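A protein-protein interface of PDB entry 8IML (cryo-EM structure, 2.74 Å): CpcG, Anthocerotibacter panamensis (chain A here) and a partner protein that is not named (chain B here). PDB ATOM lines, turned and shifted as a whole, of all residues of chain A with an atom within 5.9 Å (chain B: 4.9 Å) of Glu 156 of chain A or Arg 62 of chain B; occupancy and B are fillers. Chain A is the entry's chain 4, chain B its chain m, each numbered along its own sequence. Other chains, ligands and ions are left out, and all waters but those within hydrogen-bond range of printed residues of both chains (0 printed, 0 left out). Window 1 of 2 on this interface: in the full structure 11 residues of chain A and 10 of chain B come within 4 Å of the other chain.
Of the 11 printed residues of chain A, 2 touch a printed residue of chain B. Printed residues of chain A that touch a printed residue of chain B: Leu 79 and Glu 156. Hydrophobic or aromatic side chains of chain A within 4 Å of the printed part of chain B: Leu 79. Along chain A the printed residues that touch a printed residue of chain B span positions 79 to 156.
Among the printed residues, pairs that only touch across the chains: Leu 79 of chain A with Leu 49 of chain B (3.7 Å).
Of chain B, only Glu 59 and Arg 62 come within 4 Å of Glu 156 of chain A. Arg 62 of chain B touches just one residue of chain A: Glu 156 (2.9 Å). Printed residues of chain B within 4 Å of Leu 79 of chain A: Leu 49 (3.7 Å). Printed residues of chain A within 4 Å of Leu 49 of chain B: Leu 79 (3.7 Å). Printed residues of chain A within 4 Å of Glu 59 of chain B: Glu 156 (2.9 Å). Phe 154 of chain A touches none of the printed residues of chain B.
The guanidinium group of Arg 62 of chain B lies within salt-bridge range of the side-chain carboxylate of Glu 156 of chain A, at 2.9 Å. The side-chain carboxylate (OE2) of Glu 156 of chain A sits close to the side-chain carboxylate (OE1) of Glu 59 of chain B (2.9 Å).
The side-chain carboxylate (OE1) of Glu 59 of chain B lies within salt-bridge range of the guanidinium group (NE) of Arg 62 of chain B, 3.1 Å away.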
ATOM      1  N   LEU A  79     -11.518 -29.431  18.650  1.00  0.00           N
ATOM      2  CA  LEU A  79     -12.743 -28.813  18.184  1.00  0.00           C
ATOM      3  C   LEU A  79     -13.305 -29.592  17.000  1.00  0.00           C
ATOM      4  O   LEU A  79     -12.636 -30.441  16.408  1.00  0.00           O
ATOM      5  CB  LEU A  79     -12.487 -27.364  17.789  1.00  0.00           C
ATOM      6  CG  LEU A  79     -12.030 -26.433  18.905  1.00  0.00           C
ATOM      7  CD1 LEU A  79     -11.281 -25.259  18.324  1.00  0.00           C
ATOM      8  CD2 LEU A  79     -13.215 -25.960  19.715  1.00  0.00           C
ATOM      9  N   VAL A  80     -14.559 -29.305  16.658  1.00  0.00           N
ATOM     10  CA  VAL A  80     -15.147 -29.927  15.480  1.00  0.00           C
ATOM     11  C   VAL A  80     -14.489 -29.394  14.219  1.00  0.00           C
ATOM     12  O   VAL A  80     -14.269 -30.134  13.253  1.00  0.00           O
ATOM     13  CB  VAL A  80     -16.666 -29.709  15.456  1.00  0.00           C
ATOM     14  CG1 VAL A  80     -17.261 -30.381  14.243  1.00  0.00           C
ATOM     15  CG2 VAL A  80     -17.291 -30.230  16.725  1.00  0.00           C
ATOM     16  N   LYS A  81     -14.164 -28.101  14.206  1.00  0.00           N
ATOM     17  CA  LYS A  81     -13.447 -27.527  13.075  1.00  0.00           C
ATOM     18  C   LYS A  81     -12.106 -28.213  12.878  1.00  0.00           C
ATOM     19  O   LYS A  81     -11.716 -28.520  11.746  1.00  0.00           O
ATOM     20  CB  LYS A  81     -13.261 -26.027  13.289  1.00  0.00           C
ATOM     21  CG  LYS A  81     -12.560 -25.326  12.153  1.00  0.00           C
ATOM     22  CD  LYS A  81     -12.539 -23.829  12.364  1.00  0.00           C
ATOM     23  CE  LYS A  81     -11.593 -23.451  13.466  1.00  0.00           C
ATOM     24  NZ  LYS A  81     -10.191 -23.703  13.071  1.00  0.00           N
ATOM     25  N   ASP A  82     -11.400 -28.493  13.971  1.00  0.00           N
ATOM     26  CA  ASP A  82     -10.101 -29.139  13.859  1.00  0.00           C
ATOM     27  C   ASP A  82     -10.230 -30.604  13.476  1.00  0.00           C
ATOM     28  O   ASP A  82      -9.374 -31.129  12.764  1.00  0.00           O
ATOM     29  CB  ASP A  82      -9.334 -28.991  15.164  1.00  0.00           C
ATOM     30  CG  ASP A  82      -9.061 -27.549  15.506  1.00  0.00           C
ATOM     31  OD1 ASP A  82      -8.851 -26.753  14.568  1.00  0.00           O
ATOM     32  OD2 ASP A  82      -9.057 -27.203  16.704  1.00  0.00           O
ATOM     33  N   TYR A 150     -16.837 -20.525   6.281  1.00  0.00           N
ATOM     34  CA  TYR A 150     -16.970 -21.673   7.172  1.00  0.00           C
ATOM     35  C   TYR A 150     -17.236 -21.226   8.598  1.00  0.00           C
ATOM     36  O   TYR A 150     -18.082 -21.802   9.288  1.00  0.00           O
ATOM     37  CB  TYR A 150     -15.719 -22.549   7.115  1.00  0.00           C
ATOM     38  CG  TYR A 150     -15.812 -23.807   7.959  1.00  0.00           C
ATOM     39  CD1 TYR A 150     -15.615 -23.769   9.329  1.00  0.00           C
ATOM     40  CD2 TYR A 150     -16.096 -25.029   7.381  1.00  0.00           C
ATOM     41  CE1 TYR A 150     -15.706 -24.904  10.092  1.00  0.00           C
ATOM     42  CE2 TYR A 150     -16.180 -26.170   8.141  1.00  0.00           C
ATOM     43  CZ  TYR A 150     -15.989 -26.098   9.496  1.00  0.00           C
ATOM     44  OH  TYR A 150     -16.075 -27.224  10.270  1.00  0.00           O
ATOM     45  N   ALA A 151     -16.513 -20.209   9.063  1.00  0.00           N
ATOM     46  CA  ALA A 151     -16.711 -19.730  10.425  1.00  0.00           C
ATOM     47  C   ALA A 151     -18.104 -19.153  10.607  1.00  0.00           C
ATOM     48  O   ALA A 151     -18.724 -19.333  11.659  1.00  0.00           O
ATOM     49  CB  ALA A 151     -15.652 -18.689  10.773  1.00  0.00           C
ATOM     50  N   PHE A 154     -20.877 -22.476   9.990  1.00  0.00           N
ATOM     51  CA  PHE A 154     -20.804 -23.563  10.955  1.00  0.00           C
ATOM     52  C   PHE A 154     -20.078 -23.187  12.231  1.00  0.00           C
ATOM     53  O   PHE A 154     -20.513 -23.570  13.315  1.00  0.00           O
ATOM     54  CB  PHE A 154     -20.129 -24.781  10.325  1.00  0.00           C
ATOM     55  CG  PHE A 154     -20.613 -25.093   8.944  1.00  0.00           C
ATOM     56  CD1 PHE A 154     -21.910 -25.494   8.728  1.00  0.00           C
ATOM     57  CD2 PHE A 154     -19.773 -24.987   7.863  1.00  0.00           C
ATOM     58  CE1 PHE A 154     -22.354 -25.778   7.465  1.00  0.00           C
ATOM     59  CE2 PHE A 154     -20.220 -25.267   6.601  1.00  0.00           C
ATOM     60  CZ  PHE A 154     -21.510 -25.665   6.407  1.00  0.00           C
ATOM     61  N   GLY A 155     -18.993 -22.441  12.140  1.00  0.00           N
ATOM     62  CA  GLY A 155     -18.276 -22.038  13.326  1.00  0.00           C
ATOM     63  C   GLY A 155     -17.356 -23.118  13.846  1.00  0.00           C
ATOM     64  O   GLY A 155     -17.123 -24.152  13.222  1.00  0.00           O
ATOM     65  N   GLU A 156     -16.825 -22.861  15.039  1.00  0.00           N
ATOM     66  CA  GLU A 156     -15.845 -23.766  15.627  1.00  0.00           C
ATOM     67  C   GLU A 156     -16.502 -24.971  16.280  1.00  0.00           C
ATOM     68  O   GLU A 156     -15.804 -25.877  16.742  1.00  0.00           O
ATOM     69  CB  GLU A 156     -14.996 -23.012  16.646  1.00  0.00           C
ATOM     70  CG  GLU A 156     -13.771 -22.351  16.059  1.00  0.00           C
ATOM     71  CD  GLU A 156     -12.766 -21.942  17.113  1.00  0.00           C
ATOM     72  OE1 GLU A 156     -13.161 -21.810  18.290  1.00  0.00           O
ATOM     73  OE2 GLU A 156     -11.581 -21.753  16.766  1.00  0.00           O
ATOM     74  N   ASP A 157     -17.830 -25.000  16.337  1.00  0.00           N
ATOM     75  CA  ASP A 157     -18.530 -25.975  17.161  1.00  0.00           C
ATOM     76  C   ASP A 157     -19.401 -26.932  16.363  1.00  0.00           C
ATOM     77  O   ASP A 157     -19.620 -28.064  16.803  1.00  0.00           O
ATOM     78  CB  ASP A 157     -19.393 -25.243  18.190  1.00  0.00           C
ATOM     79  CG  ASP A 157     -20.259 -24.162  17.563  1.00  0.00           C
ATOM     80  OD1 ASP A 157     -19.880 -23.645  16.492  1.00  0.00           O
ATOM     81  OD2 ASP A 157     -21.314 -23.826  18.140  1.00  0.00           O
ATOM     82  N   THR A 158     -19.904 -26.509  15.212  1.00  0.00           N
ATOM     83  CA  THR A 158     -20.843 -27.296  14.430  1.00  0.00           C
ATOM     84  C   THR A 158     -20.125 -28.059  13.326  1.00  0.00           C
ATOM     85  O   THR A 158     -19.120 -27.604  12.778  1.00  0.00           O
ATOM     86  CB  THR A 158     -21.909 -26.381  13.827  1.00  0.00           C
ATOM     87  OG1 THR A 158     -22.581 -25.675  14.876  1.00  0.00           O
ATOM     88  CG2 THR A 158     -22.919 -27.158  13.032  1.00  0.00           C
ATOM     89  N   LEU B  49      -9.058 -24.438  26.050  1.00  0.00           N
ATOM     90  CA  LEU B  49      -8.868 -24.635  24.622  1.00  0.00           C
ATOM     91  C   LEU B  49      -7.386 -24.817  24.340  1.00  0.00           C
ATOM     92  O   LEU B  49      -6.569 -23.981  24.734  1.00  0.00           O
ATOM     93  CB  LEU B  49      -9.426 -23.445  23.845  1.00  0.00           C
ATOM     94  CG  LEU B  49      -8.963 -23.229  22.410  1.00  0.00           C
ATOM     95  CD1 LEU B  49      -9.581 -24.255  21.474  1.00  0.00           C
ATOM     96  CD2 LEU B  49      -9.325 -21.819  21.988  1.00  0.00           C
ATOM     97  N   PRO B  58      -3.087 -16.604  15.646  1.00  0.00           N
ATOM     98  CA  PRO B  58      -4.421 -16.385  15.068  1.00  0.00           C
ATOM     99  C   PRO B  58      -5.547 -16.728  16.019  1.00  0.00           C
ATOM    100  O   PRO B  58      -6.575 -16.043  16.017  1.00  0.00           O
ATOM    101  CB  PRO B  58      -4.420 -17.298  13.837  1.00  0.00           C
ATOM    102  CG  PRO B  58      -2.993 -17.454  13.493  1.00  0.00           C
ATOM    103  CD  PRO B  58      -2.293 -17.519  14.807  1.00  0.00           C
ATOM    104  N   GLU B  59      -5.382 -17.762  16.843  1.00  0.00           N
ATOM    105  CA  GLU B  59      -6.436 -18.114  17.785  1.00  0.00           C
ATOM    106  C   GLU B  59      -6.642 -17.013  18.814  1.00  0.00           C
ATOM    107  O   GLU B  59      -7.784 -16.663  19.134  1.00  0.00           O
ATOM    108  CB  GLU B  59      -6.115 -19.440  18.469  1.00  0.00           C
ATOM    109  CG  GLU B  59      -6.667 -20.636  17.722  1.00  0.00           C
ATOM    110  CD  GLU B  59      -8.152 -20.817  17.933  1.00  0.00           C
ATOM    111  OE1 GLU B  59      -8.921 -20.596  16.975  1.00  0.00           O
ATOM    112  OE2 GLU B  59      -8.552 -21.180  19.054  1.00  0.00           O
ATOM    113  N   MET B  60      -5.555 -16.437  19.336  1.00  0.00           N
ATOM    114  CA  MET B  60      -5.738 -15.340  20.283  1.00  0.00           C
ATOM    115  C   MET B  60      -6.269 -14.082  19.610  1.00  0.00           C
ATOM    116  O   MET B  60      -7.037 -13.337  20.229  1.00  0.00           O
ATOM    117  CB  MET B  60      -4.447 -15.023  21.025  1.00  0.00           C
ATOM    118  CG  MET B  60      -3.987 -16.112  21.953  1.00  0.00           C
ATOM    119  SD  MET B  60      -2.432 -15.622  22.689  1.00  0.00           S
ATOM    120  CE  MET B  60      -3.029 -14.313  23.753  1.00  0.00           C
ATOM    121  N   ILE B  61      -5.874 -13.816  18.365  1.00  0.00           N
ATOM    122  CA  ILE B  61      -6.466 -12.695  17.640  1.00  0.00           C
ATOM    123  C   ILE B  61      -7.967 -12.894  17.507  1.00  0.00           C
ATOM    124  O   ILE B  61      -8.753 -11.958  17.689  1.00  0.00           O
ATOM    125  CB  ILE B  61      -5.801 -12.516  16.263  1.00  0.00           C
ATOM    126  CG1 ILE B  61      -4.298 -12.302  16.403  1.00  0.00           C
ATOM    127  CG2 ILE B  61      -6.435 -11.361  15.513  1.00  0.00           C
ATOM    128  CD1 ILE B  61      -3.545 -12.453  15.104  1.00  0.00           C
ATOM    129  N   ARG B  62      -8.386 -14.118  17.186  1.00  0.00           N
ATOM    130  CA  ARG B  62      -9.809 -14.418  17.088  1.00  0.00           C
ATOM    131  C   ARG B  62     -10.506 -14.228  18.427  1.00  0.00           C
ATOM    132  O   ARG B  62     -11.612 -13.682  18.485  1.00  0.00           O
ATOM    133  CB  ARG B  62     -10.000 -15.847  16.584  1.00  0.00           C
ATOM    134  CG  ARG B  62     -11.315 -16.090  15.878  1.00  0.00           C
ATOM    135  CD  ARG B  62     -11.447 -17.549  15.478  1.00  0.00           C
ATOM    136  NE  ARG B  62     -11.128 -18.452  16.580  1.00  0.00           N
ATOM    137  CZ  ARG B  62     -11.883 -18.621  17.662  1.00  0.00           C
ATOM    138  NH1 ARG B  62     -13.022 -17.958  17.797  1.00  0.00           N
ATOM    139  NH2 ARG B  62     -11.498 -19.465  18.610  1.00  0.00           N
ATOM    140  N   LEU B  63      -9.877 -14.675  19.516  1.00  0.00           N
ATOM    141  CA  LEU B  63     -10.496 -14.533  20.830  1.00  0.00           C
ATOM    142  C   LEU B  63     -10.650 -13.071  21.219  1.00  0.00           C
ATOM    143  O   LEU B  63     -11.689 -12.669  21.758  1.00  0.00           O
ATOM    144  CB  LEU B  63      -9.679 -15.280  21.881  1.00  0.00           C
ATOM    145  CG  LEU B  63      -9.617 -16.794  21.690  1.00  0.00           C
ATOM    146  CD1 LEU B  63      -8.750 -17.439  22.755  1.00  0.00           C
ATOM    147  CD2 LEU B  63     -11.015 -17.382  21.694  1.00  0.00           C
ATOM    148  N   HIS B  64      -9.627 -12.258  20.956  1.00  0.00           N
ATOM    149  CA  HIS B  64      -9.680 -10.852  21.343  1.00  0.00           C
ATOM    150  C   HIS B  64     -10.640 -10.065  20.461  1.00  0.00           C
ATOM    151  O   HIS B  64     -11.404  -9.232  20.961  1.00  0.00           O
ATOM    152  CB  HIS B  64      -8.279 -10.253  21.299  1.00  0.00           C
ATOM    153  CG  HIS B  64      -7.332 -10.886  22.268  1.00  0.00           C
ATOM    154  ND1 HIS B  64      -7.756 -11.502  23.424  1.00  0.00           N
ATOM    155  CD2 HIS B  64      -5.985 -11.017  22.243  1.00  0.00           C
ATOM    156  CE1 HIS B  64      -6.710 -11.973  24.079  1.00  0.00           C
ATOM    157  NE2 HIS B  64      -5.624 -11.692  23.383  1.00  0.00           N
ATOM    158  N   GLN B  65     -10.617 -10.306  19.148  1.00  0.00           N
ATOM    159  CA  GLN B  65     -11.556  -9.637  18.258  1.00  0.00           C
ATOM    160  C   GLN B  65     -12.988 -10.048  18.565  1.00  0.00           C
ATOM    161  O   GLN B  65     -13.908  -9.225  18.498  1.00  0.00           O
ATOM    162  CB  GLN B  65     -11.207  -9.945  16.801  1.00  0.00           C
ATOM    163  CG  GLN B  65     -12.244  -9.470  15.797  1.00  0.00           C
ATOM    164  CD  GLN B  65     -12.103  -7.997  15.455  1.00  0.00           C
ATOM    165  OE1 GLN B  65     -11.564  -7.211  16.235  1.00  0.00           O
ATOM    166  NE2 GLN B  65     -12.597  -7.614  14.283  1.00  0.00           N
ATOM    167  N   SER B  66     -13.195 -11.318  18.914  1.00  0.00           N
ATOM    168  CA  SER B  66     -14.530 -11.804  19.228  1.00  0.00           C
ATOM    169  C   SER B  66     -15.074 -11.217  20.522  1.00  0.00           C
ATOM    170  O   SER B  66     -16.277 -11.329  20.778  1.00  0.00           O
ATOM    171  CB  SER B  66     -14.517 -13.329  19.308  1.00  0.00           C
ATOM    172  OG  SER B  66     -15.805 -13.825  19.612  1.00  0.00           O
